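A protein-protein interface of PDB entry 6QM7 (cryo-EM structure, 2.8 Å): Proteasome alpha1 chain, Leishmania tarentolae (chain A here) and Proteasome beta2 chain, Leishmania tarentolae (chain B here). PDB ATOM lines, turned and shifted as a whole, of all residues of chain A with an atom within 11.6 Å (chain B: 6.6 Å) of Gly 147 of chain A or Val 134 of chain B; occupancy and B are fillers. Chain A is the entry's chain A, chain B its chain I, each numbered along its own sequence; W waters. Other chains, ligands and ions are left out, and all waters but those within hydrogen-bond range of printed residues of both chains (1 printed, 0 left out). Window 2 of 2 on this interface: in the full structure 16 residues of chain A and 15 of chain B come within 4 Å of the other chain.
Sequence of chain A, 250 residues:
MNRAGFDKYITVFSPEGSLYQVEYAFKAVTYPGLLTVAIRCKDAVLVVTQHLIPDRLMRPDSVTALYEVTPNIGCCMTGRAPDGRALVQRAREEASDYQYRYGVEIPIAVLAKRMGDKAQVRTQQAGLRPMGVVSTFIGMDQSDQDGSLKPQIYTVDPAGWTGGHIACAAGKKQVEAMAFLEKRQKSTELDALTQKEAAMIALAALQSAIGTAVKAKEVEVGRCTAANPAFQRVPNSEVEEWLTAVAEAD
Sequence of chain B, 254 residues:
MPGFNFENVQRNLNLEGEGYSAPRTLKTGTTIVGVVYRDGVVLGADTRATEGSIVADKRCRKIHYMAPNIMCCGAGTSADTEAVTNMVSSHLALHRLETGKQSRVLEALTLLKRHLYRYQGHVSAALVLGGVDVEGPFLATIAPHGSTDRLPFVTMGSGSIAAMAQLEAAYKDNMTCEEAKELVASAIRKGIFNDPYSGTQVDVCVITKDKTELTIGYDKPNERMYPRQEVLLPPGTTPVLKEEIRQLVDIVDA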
ATOM      1  N   VAL A 104      22.890   6.270  23.459  1.00  0.00           N
ATOM      2  CA  VAL A 104      22.276   7.503  22.891  1.00  0.00           C
ATOM      3  C   VAL A 104      21.922   7.214  21.437  1.00  0.00           C
ATOM      4  O   VAL A 104      22.538   6.317  20.865  1.00  0.00           O
ATOM      5  CB  VAL A 104      23.193   8.732  23.029  1.00  0.00           C
ATOM      6  CG1 VAL A 104      23.546   9.011  24.483  1.00  0.00           C
ATOM      7  CG2 VAL A 104      24.458   8.617  22.195  1.00  0.00           C
ATOM      8  N   GLU A 105      20.941   7.938  20.895  1.00  0.00           N
ATOM      9  CA  GLU A 105      20.554   7.863  19.465  1.00  0.00           C
ATOM     10  C   GLU A 105      21.777   8.214  18.617  1.00  0.00           C
ATOM     11  O   GLU A 105      22.486   9.178  18.963  1.00  0.00           O
ATOM     12  CB  GLU A 105      19.391   8.804  19.140  1.00  0.00           C
ATOM     13  CG  GLU A 105      18.016   8.214  19.435  1.00  0.00           C
ATOM     14  CD  GLU A 105      16.941   8.424  18.369  1.00  0.00           C
ATOM     15  OE1 GLU A 105      17.290   8.539  17.164  1.00  0.00           O
ATOM     16  OE2 GLU A 105      15.743   8.450  18.737  1.00  0.00           O
ATOM     17  N   PRO A 107      23.804  10.062  16.069  1.00  0.00           N
ATOM     18  CA  PRO A 107      23.742  11.326  15.348  1.00  0.00           C
ATOM     19  C   PRO A 107      23.673  11.087  13.843  1.00  0.00           C
ATOM     20  O   PRO A 107      24.370  10.236  13.381  1.00  0.00           O
ATOM     21  CB  PRO A 107      25.074  12.021  15.649  1.00  0.00           C
ATOM     22  CG  PRO A 107      25.521  11.398  16.931  1.00  0.00           C
ATOM     23  CD  PRO A 107      25.014   9.972  16.893  1.00  0.00           C
ATOM     24  N   MET A 140      17.066  16.230  12.808  1.00  0.00           N
ATOM     25  CA  MET A 140      17.648  17.245  13.699  1.00  0.00           C
ATOM     26  C   MET A 140      18.958  16.689  14.251  1.00  0.00           C
ATOM     27  O   MET A 140      19.092  15.457  14.338  1.00  0.00           O
ATOM     28  CB  MET A 140      16.679  17.567  14.840  1.00  0.00           C
ATOM     29  CG  MET A 140      15.412  18.327  14.420  1.00  0.00           C
ATOM     30  SD  MET A 140      15.311  18.915  12.692  1.00  0.00           S
ATOM     31  CE  MET A 140      15.406  20.685  12.948  1.00  0.00           C
ATOM     32  N   ASP A 141      19.873  17.591  14.594  1.00  0.00           N
ATOM     33  CA  ASP A 141      21.152  17.298  15.281  1.00  0.00           C
ATOM     34  C   ASP A 141      21.333  18.309  16.418  1.00  0.00           C
ATOM     35  O   ASP A 141      21.322  19.519  16.120  1.00  0.00           O
ATOM     36  CB  ASP A 141      22.301  17.361  14.275  1.00  0.00           C
ATOM     37  CG  ASP A 141      23.673  17.434  14.928  1.00  0.00           C
ATOM     38  OD1 ASP A 141      24.175  16.368  15.379  1.00  0.00           O
ATOM     39  OD2 ASP A 141      24.214  18.563  15.005  1.00  0.00           O
ATOM     40  N   GLN A 142      21.531  17.847  17.655  1.00  0.00           N
ATOM     41  CA  GLN A 142      21.700  18.740  18.831  1.00  0.00           C
ATOM     42  C   GLN A 142      23.085  19.405  18.766  1.00  0.00           C
ATOM     43  O   GLN A 142      24.099  18.679  18.791  1.00  0.00           O
ATOM     44  CB  GLN A 142      21.477  17.976  20.137  1.00  0.00           C
ATOM     45  CG  GLN A 142      21.140  18.887  21.310  1.00  0.00           C
ATOM     46  CD  GLN A 142      20.744  18.126  22.553  1.00  0.00           C
ATOM     47  OE1 GLN A 142      21.004  16.933  22.684  1.00  0.00           O
ATOM     48  NE2 GLN A 142      20.096  18.815  23.478  1.00  0.00           N
ATOM     49  N   SER A 143      23.111  20.736  18.646  1.00  0.00           N
ATOM     50  CA  SER A 143      24.317  21.592  18.812  1.00  0.00           C
ATOM     51  C   SER A 143      24.787  21.496  20.263  1.00  0.00           C
ATOM     52  O   SER A 143      23.962  21.734  21.155  1.00  0.00           O
ATOM     53  CB  SER A 143      24.044  23.035  18.415  1.00  0.00           C
ATOM     54  OG  SER A 143      24.941  23.937  19.057  1.00  0.00           O
ATOM     55  N   ASP A 144      26.065  21.174  20.482  1.00  0.00           N
ATOM     56  CA  ASP A 144      26.646  20.959  21.838  1.00  0.00           C
ATOM     57  C   ASP A 144      26.943  22.313  22.505  1.00  0.00           C
ATOM     58  O   ASP A 144      27.141  22.311  23.732  1.00  0.00           O
ATOM     59  CB  ASP A 144      27.856  20.009  21.801  1.00  0.00           C
ATOM     60  CG  ASP A 144      28.963  20.370  20.818  1.00  0.00           C
ATOM     61  OD1 ASP A 144      28.761  21.312  20.014  1.00  0.00           O
ATOM     62  OD2 ASP A 144      30.022  19.701  20.854  1.00  0.00           O
ATOM     63  N   GLN A 145      26.933  23.422  21.749  1.00  0.00           N
ATOM     64  CA  GLN A 145      27.233  24.794  22.250  1.00  0.00           C
ATOM     65  C   GLN A 145      26.088  25.329  23.124  1.00  0.00           C
ATOM     66  O   GLN A 145      26.405  25.860  24.200  1.00  0.00           O
ATOM     67  CB  GLN A 145      27.520  25.743  21.087  1.00  0.00           C
ATOM     68  CG  GLN A 145      28.788  25.379  20.324  1.00  0.00           C
ATOM     69  CD  GLN A 145      29.132  26.365  19.232  1.00  0.00           C
ATOM     70  OE1 GLN A 145      28.270  27.055  18.690  1.00  0.00           O
ATOM     71  NE2 GLN A 145      30.410  26.436  18.894  1.00  0.00           N
ATOM     72  N   ASP A 146      24.827  25.220  22.684  1.00  0.00           N
ATOM     73  CA  ASP A 146      23.640  25.782  23.398  1.00  0.00           C
ATOM     74  C   ASP A 146      22.529  24.741  23.632  1.00  0.00           C
ATOM     75  O   ASP A 146      21.640  25.049  24.452  1.00  0.00           O
ATOM     76  CB  ASP A 146      23.072  27.013  22.675  1.00  0.00           C
ATOM     77  CG  ASP A 146      22.664  26.806  21.223  1.00  0.00           C
ATOM     78  OD1 ASP A 146      22.030  27.724  20.667  1.00  0.00           O
ATOM     79  OD2 ASP A 146      22.995  25.743  20.649  1.00  0.00           O
ATOM     80  N   GLY A 147      22.544  23.585  22.952  1.00  0.00           N
ATOM     81  CA  GLY A 147      21.541  22.506  23.111  1.00  0.00           C
ATOM     82  C   GLY A 147      20.422  22.594  22.089  1.00  0.00           C
ATOM     83  O   GLY A 147      19.599  21.654  22.043  1.00  0.00           O
ATOM     84  N   SER A 148      20.396  23.676  21.297  1.00  0.00           N
ATOM     85  CA  SER A 148      19.438  23.909  20.186  1.00  0.00           C
ATOM     86  C   SER A 148      19.584  22.788  19.155  1.00  0.00           C
ATOM     87  O   SER A 148      20.729  22.453  18.809  1.00  0.00           O
ATOM     88  CB  SER A 148      19.646  25.252  19.535  1.00  0.00           C
ATOM     89  OG  SER A 148      20.783  25.228  18.680  1.00  0.00           O
ATOM     90  N   LEU A 149      18.456  22.225  18.716  1.00  0.00           N
ATOM     91  CA  LEU A 149      18.392  21.293  17.568  1.00  0.00           C
ATOM     92  C   LEU A 149      18.572  22.116  16.301  1.00  0.00           C
ATOM     93  O   LEU A 149      18.061  23.243  16.276  1.00  0.00           O
ATOM     94  CB  LEU A 149      17.038  20.579  17.572  1.00  0.00           C
ATOM     95  CG  LEU A 149      16.796  19.627  18.742  1.00  0.00           C
ATOM     96  CD1 LEU A 149      15.473  18.892  18.560  1.00  0.00           C
ATOM     97  CD2 LEU A 149      17.936  18.632  18.888  1.00  0.00           C
ATOM     98  N   LYS A 150      19.294  21.595  15.312  1.00  0.00           N
ATOM     99  CA  LYS A 150      19.342  22.221  13.969  1.00  0.00           C
ATOM    100  C   LYS A 150      19.146  21.138  12.916  1.00  0.00           C
ATOM    101  O   LYS A 150      19.572  20.002  13.085  1.00  0.00           O
ATOM    102  CB  LYS A 150      20.586  23.105  13.803  1.00  0.00           C
ATOM    103  CG  LYS A 150      21.805  22.503  13.115  1.00  0.00           C
ATOM    104  CD  LYS A 150      22.922  22.100  14.067  1.00  0.00           C
ATOM    105  CE  LYS A 150      24.272  21.976  13.383  1.00  0.00           C
ATOM    106  NZ  LYS A 150      25.348  21.655  14.353  1.00  0.00           N
ATOM    107  N   PRO A 151      18.440  21.464  11.817  1.00  0.00           N
ATOM    108  CA  PRO A 151      18.167  20.502  10.756  1.00  0.00           C
ATOM    109  C   PRO A 151      19.394  20.136   9.903  1.00  0.00           C
ATOM    110  O   PRO A 151      20.224  20.997   9.614  1.00  0.00           O
ATOM    111  CB  PRO A 151      17.121  21.224   9.897  1.00  0.00           C
ATOM    112  CG  PRO A 151      17.408  22.676  10.112  1.00  0.00           C
ATOM    113  CD  PRO A 151      17.834  22.774  11.555  1.00  0.00           C
ATOM    114  N   THR A 225      11.302  18.652  12.462  1.00  0.00           N
ATOM    115  CA  THR A 225      11.274  20.066  12.917  1.00  0.00           C
ATOM    116  C   THR A 225      11.991  20.153  14.266  1.00  0.00           C
ATOM    117  O   THR A 225      12.151  19.105  14.900  1.00  0.00           O
ATOM    118  CB  THR A 225       9.842  20.611  12.975  1.00  0.00           C
ATOM    119  OG1 THR A 225       9.254  20.323  14.244  1.00  0.00           O
ATOM    120  CG2 THR A 225       8.956  20.057  11.881  1.00  0.00           C
ATOM    121  N   ALA A 226      12.411  21.354  14.674  1.00  0.00           N
ATOM    122  CA  ALA A 226      12.983  21.633  16.013  1.00  0.00           C
ATOM    123  C   ALA A 226      11.932  21.299  17.081  1.00  0.00           C
ATOM    124  O   ALA A 226      12.282  20.620  18.068  1.00  0.00           O
ATOM    125  CB  ALA A 226      13.435  23.073  16.086  1.00  0.00           C
ATOM    126  N   ALA A 227      10.690  21.751  16.854  1.00  0.00           N
ATOM    127  CA  ALA A 227       9.490  21.529  17.699  1.00  0.00           C
ATOM    128  C   ALA A 227       9.225  20.027  17.857  1.00  0.00           C
ATOM    129  O   ALA A 227       9.164  19.553  19.011  1.00  0.00           O
ATOM    130  CB  ALA A 227       8.294  22.225  17.087  1.00  0.00           C
ATOM    131  N   PRO A 229      11.044  16.801  16.619  1.00  0.00           N
ATOM    132  CA  PRO A 229      12.254  16.285  15.967  1.00  0.00           C
ATOM    133  C   PRO A 229      12.109  14.905  15.312  1.00  0.00           C
ATOM    134  O   PRO A 229      12.950  14.578  14.492  1.00  0.00           O
ATOM    135  CB  PRO A 229      13.285  16.221  17.103  1.00  0.00           C
ATOM    136  CG  PRO A 229      12.451  16.039  18.346  1.00  0.00           C
ATOM    137  CD  PRO A 229      11.179  16.822  18.086  1.00  0.00           C
ATOM    138  N   ASN B  69      35.497  17.098  29.149  1.00  0.00           N
ATOM    139  CA  ASN B  69      34.319  17.475  29.972  1.00  0.00           C
ATOM    140  C   ASN B  69      33.872  16.336  30.894  1.00  0.00           C
ATOM    141  O   ASN B  69      32.723  16.402  31.344  1.00  0.00           O
ATOM    142  CB  ASN B  69      33.128  17.838  29.085  1.00  0.00           C
ATOM    143  CG  ASN B  69      32.670  16.688  28.210  1.00  0.00           C
ATOM    144  OD1 ASN B  69      33.499  16.006  27.612  1.00  0.00           O
ATOM    145  ND2 ASN B  69      31.366  16.473  28.123  1.00  0.00           N
ATOM    146  N   GLN B 102      31.388  17.020  21.433  1.00  0.00           N
ATOM    147  CA  GLN B 102      31.897  16.801  22.817  1.00  0.00           C
ATOM    148  C   GLN B 102      31.265  15.509  23.350  1.00  0.00           C
ATOM    149  O   GLN B 102      30.082  15.293  23.096  1.00  0.00           O
ATOM    150  CB  GLN B 102      31.687  18.046  23.693  1.00  0.00           C
ATOM    151  CG  GLN B 102      30.743  17.866  24.874  1.00  0.00           C
ATOM    152  CD  GLN B 102      30.649  19.102  25.745  1.00  0.00           C
ATOM    153  OE1 GLN B 102      29.558  19.624  25.990  1.00  0.00           O
ATOM    154  NE2 GLN B 102      31.791  19.576  26.226  1.00  0.00           N
ATOM    155  N   SER B 103      32.049  14.653  23.998  1.00  0.00           N
ATOM    156  CA  SER B 103      31.576  13.332  24.474  1.00  0.00           C
ATOM    157  C   SER B 103      30.527  13.574  25.546  1.00  0.00           C
ATOM    158  O   SER B 103      30.746  14.452  26.394  1.00  0.00           O
ATOM    159  CB  SER B 103      32.680  12.421  24.974  1.00  0.00           C
ATOM    160  OG  SER B 103      33.771  13.156  25.491  1.00  0.00           O
ATOM    161  N   ARG B 104      29.411  12.856  25.452  1.00  0.00           N
ATOM    162  CA  ARG B 104      28.320  12.891  26.452  1.00  0.00           C
ATOM    163  C   ARG B 104      28.686  11.938  27.578  1.00  0.00           C
ATOM    164  O   ARG B 104      29.353  10.930  27.315  1.00  0.00           O
ATOM    165  CB  ARG B 104      26.983  12.553  25.802  1.00  0.00           C
ATOM    166  CG  ARG B 104      26.397  13.739  25.057  1.00  0.00           C
ATOM    167  CD  ARG B 104      25.932  13.348  23.672  1.00  0.00           C
ATOM    168  NE  ARG B 104      25.164  14.437  23.096  1.00  0.00           N
ATOM    169  CZ  ARG B 104      23.904  14.718  23.396  1.00  0.00           C
ATOM    170  NH1 ARG B 104      23.310  15.741  22.803  1.00  0.00           N
ATOM    171  NH2 ARG B 104      23.232  13.981  24.272  1.00  0.00           N
ATOM    172  N   VAL B 132      30.094  17.196  32.421  1.00  0.00           N
ATOM    173  CA  VAL B 132      29.101  18.209  32.009  1.00  0.00           C
ATOM    174  C   VAL B 132      29.060  18.227  30.492  1.00  0.00           C
ATOM    175  O   VAL B 132      30.004  18.743  29.863  1.00  0.00           O
ATOM    176  CB  VAL B 132      29.441  19.579  32.596  1.00  0.00           C
ATOM    177  CG1 VAL B 132      28.345  20.576  32.288  1.00  0.00           C
ATOM    178  CG2 VAL B 132      29.666  19.487  34.095  1.00  0.00           C
ATOM    179  N   ASP B 133      28.001  17.645  29.953  1.00  0.00           N
ATOM    180  CA  ASP B 133      27.679  17.665  28.512  1.00  0.00           C
ATOM    181  C   ASP B 133      26.648  18.781  28.319  1.00  0.00           C
ATOM    182  O   ASP B 133      26.473  19.599  29.242  1.00  0.00           O
ATOM    183  CB  ASP B 133      27.287  16.255  28.043  1.00  0.00           C
ATOM    184  CG  ASP B 133      26.217  15.513  28.855  1.00  0.00           C
ATOM    185  OD1 ASP B 133      25.413  16.183  29.552  1.00  0.00           O
ATOM    186  OD2 ASP B 133      26.190  14.251  28.793  1.00  0.00           O
ATOM    187  N   VAL B 134      26.026  18.827  27.147  1.00  0.00           N
ATOM    188  CA  VAL B 134      24.981  19.822  26.779  1.00  0.00           C
ATOM    189  C   VAL B 134      23.702  19.597  27.596  1.00  0.00           C
ATOM    190  O   VAL B 134      23.007  20.592  27.871  1.00  0.00           O
ATOM    191  CB  VAL B 134      24.707  19.770  25.267  1.00  0.00           C
ATOM    192  CG1 VAL B 134      24.132  18.429  24.799  1.00  0.00           C
ATOM    193  CG2 VAL B 134      23.812  20.924  24.857  1.00  0.00           C
ATOM    194  N   GLU B 135      23.395  18.345  27.952  1.00  0.00           N
ATOM    195  CA  GLU B 135      22.242  17.982  28.825  1.00  0.00           C
ATOM    196  C   GLU B 135      22.466  18.478  30.266  1.00  0.00           C
ATOM    197  O   GLU B 135      21.514  18.383  31.065  1.00  0.00           O
ATOM    198  CB  GLU B 135      21.997  16.465  28.834  1.00  0.00           C
ATOM    199  CG  GLU B 135      20.782  16.001  28.036  1.00  0.00           C
ATOM    200  CD  GLU B 135      21.088  15.381  26.682  1.00  0.00           C
ATOM    201  OE1 GLU B 135      21.894  14.421  26.641  1.00  0.00           O
ATOM    202  OE2 GLU B 135      20.523  15.858  25.668  1.00  0.00           O
ATOM    203  N   GLY B 136      23.677  18.928  30.608  1.00  0.00           N
ATOM    204  CA  GLY B 136      24.002  19.558  31.903  1.00  0.00           C
ATOM    205  C   GLY B 136      24.893  18.672  32.766  1.00  0.00           C
ATOM    206  O   GLY B 136      25.529  17.753  32.267  1.00  0.00           O
ATOM    207  N   LYS B 209      30.721  23.411  32.636  1.00  0.00           N
ATOM    208  CA  LYS B 209      30.284  23.364  31.212  1.00  0.00           C
ATOM    209  C   LYS B 209      31.488  23.634  30.297  1.00  0.00           C
ATOM    210  O   LYS B 209      31.663  22.878  29.328  1.00  0.00           O
ATOM    211  CB  LYS B 209      29.091  24.323  31.066  1.00  0.00           C
ATOM    212  CG  LYS B 209      28.940  25.089  29.758  1.00  0.00           C
ATOM    213  CD  LYS B 209      28.232  24.316  28.674  1.00  0.00           C
ATOM    214  CE  LYS B 209      28.015  25.166  27.441  1.00  0.00           C
ATOM    215  NZ  LYS B 209      27.228  24.442  26.417  1.00  0.00           N
HETATM  216  O   HOH W   1      24.837  17.074  20.794  1.00  0.00           O
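Printed residues of chain A that touch a printed residue of chain B: Gln 142, Ser 143, Asp 144, Gln 145 and Gly 147. Of the 10 printed residues of chain B, 5 touch a printed residue of chain A. Printed residues of chain B that touch a printed residue of chain A: Gln 102, Arg 104, Val 134, Glu 135 and Lys 209. Hydrophobic or aromatic side chains of chain B that line the printed part of chain A: Val 134. Among the printed residues, 8 pairs touch across the chains.
NE2 of Gln 142 of chain A is in hydrogen-bond range of O of Gly 147 of chain A (3.2 Å). N of Gln 145 of chain A sits close to OG of Ser 143 of chain A (3.4 Å). The side-chain hydroxyl of Ser 143 of chain A lies within hydrogen-bond range of the side-chain carboxylate of Asp 146 of chain A. The backbone NH (N) of Ser 143 of chain A is in hydrogen-bond range of the backbone carbonyl oxygen (O) of Ser 148 of chain A (2.9 Å). The side-chain carboxylate (OE1) of Glu 135 of chain B lies within salt-bridge range of the guanidinium group (NH2) of Arg 104 of chain B, at 2.8 Å. OD1 of Asp 133 of chain B sits close to N of Glu 135 of chain B.
Water W1 bridges the backbone carbonyl oxygen of Gln 142 of chain A (2.7 Å) and the guanidinium group of Arg 104 of chain B (2.9 Å).
CG2 of Val 134 of chain B touches O of Ser 143 of chain A, at 3.8 Å. Asp 144 of chain A touches Val 134 of chain B (O to CG2, 3.8 Å). CA of Gly 147 of chain A touches CG2 of Val 134 of chain B, 3.3 Å away.
The side-chain amide oxygen (OE1) of Gln 142 of chain A sits at hydrogen-bond distance from the guanidinium group (NH1) of Arg 104 of chain B, 2.6 Å away. OE1 of Gln 142 of chain A sits close to OE2 of Glu 135 of chain B. OD2 of Asp 144 of chain A sits at hydrogen-bond distance from N of Gln 102 of chain B (3.1 Å). The backbone carbonyl oxygen of Asp 144 of chain A sits at hydrogen-bond distance from the side-chain amino group of Lys 209 of chain B (3.4 Å). The side-chain amino group (NZ) of Lys 209 of chain B sits at hydrogen-bond distance from the backbone carbonyl oxygen (O) of Gln 145 of chain A (2.8 Å).
Gly 147 of chain A touches one residue of chain B. Val 134 of chain B touches just these residues of chain A: Ser 143 (3.8 Å), Asp 144 (3.8 Å) and Gly 147 (3.3 Å). Glu 135 of chain B touches just one residue of chain A: Gln 142. No residue of chain A comes within 4 Å of Gly 136 of chain B. Printed residues of chain B within 4 Å of Ser 143 of chain A: Val 134 (3.8 Å). Of the printed residues of chain B, Asp 144 of chain A touches Gln 102, Val 134 and Lys 209. Ser 148 of chain A touches none of the printed residues of chain B. Pro 107 of chain A touches none of the printed residues of chain B. The nearest residue of chain A that does not touch Val 134 of chain B is Gln 142 of chain A (4.1 Å).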
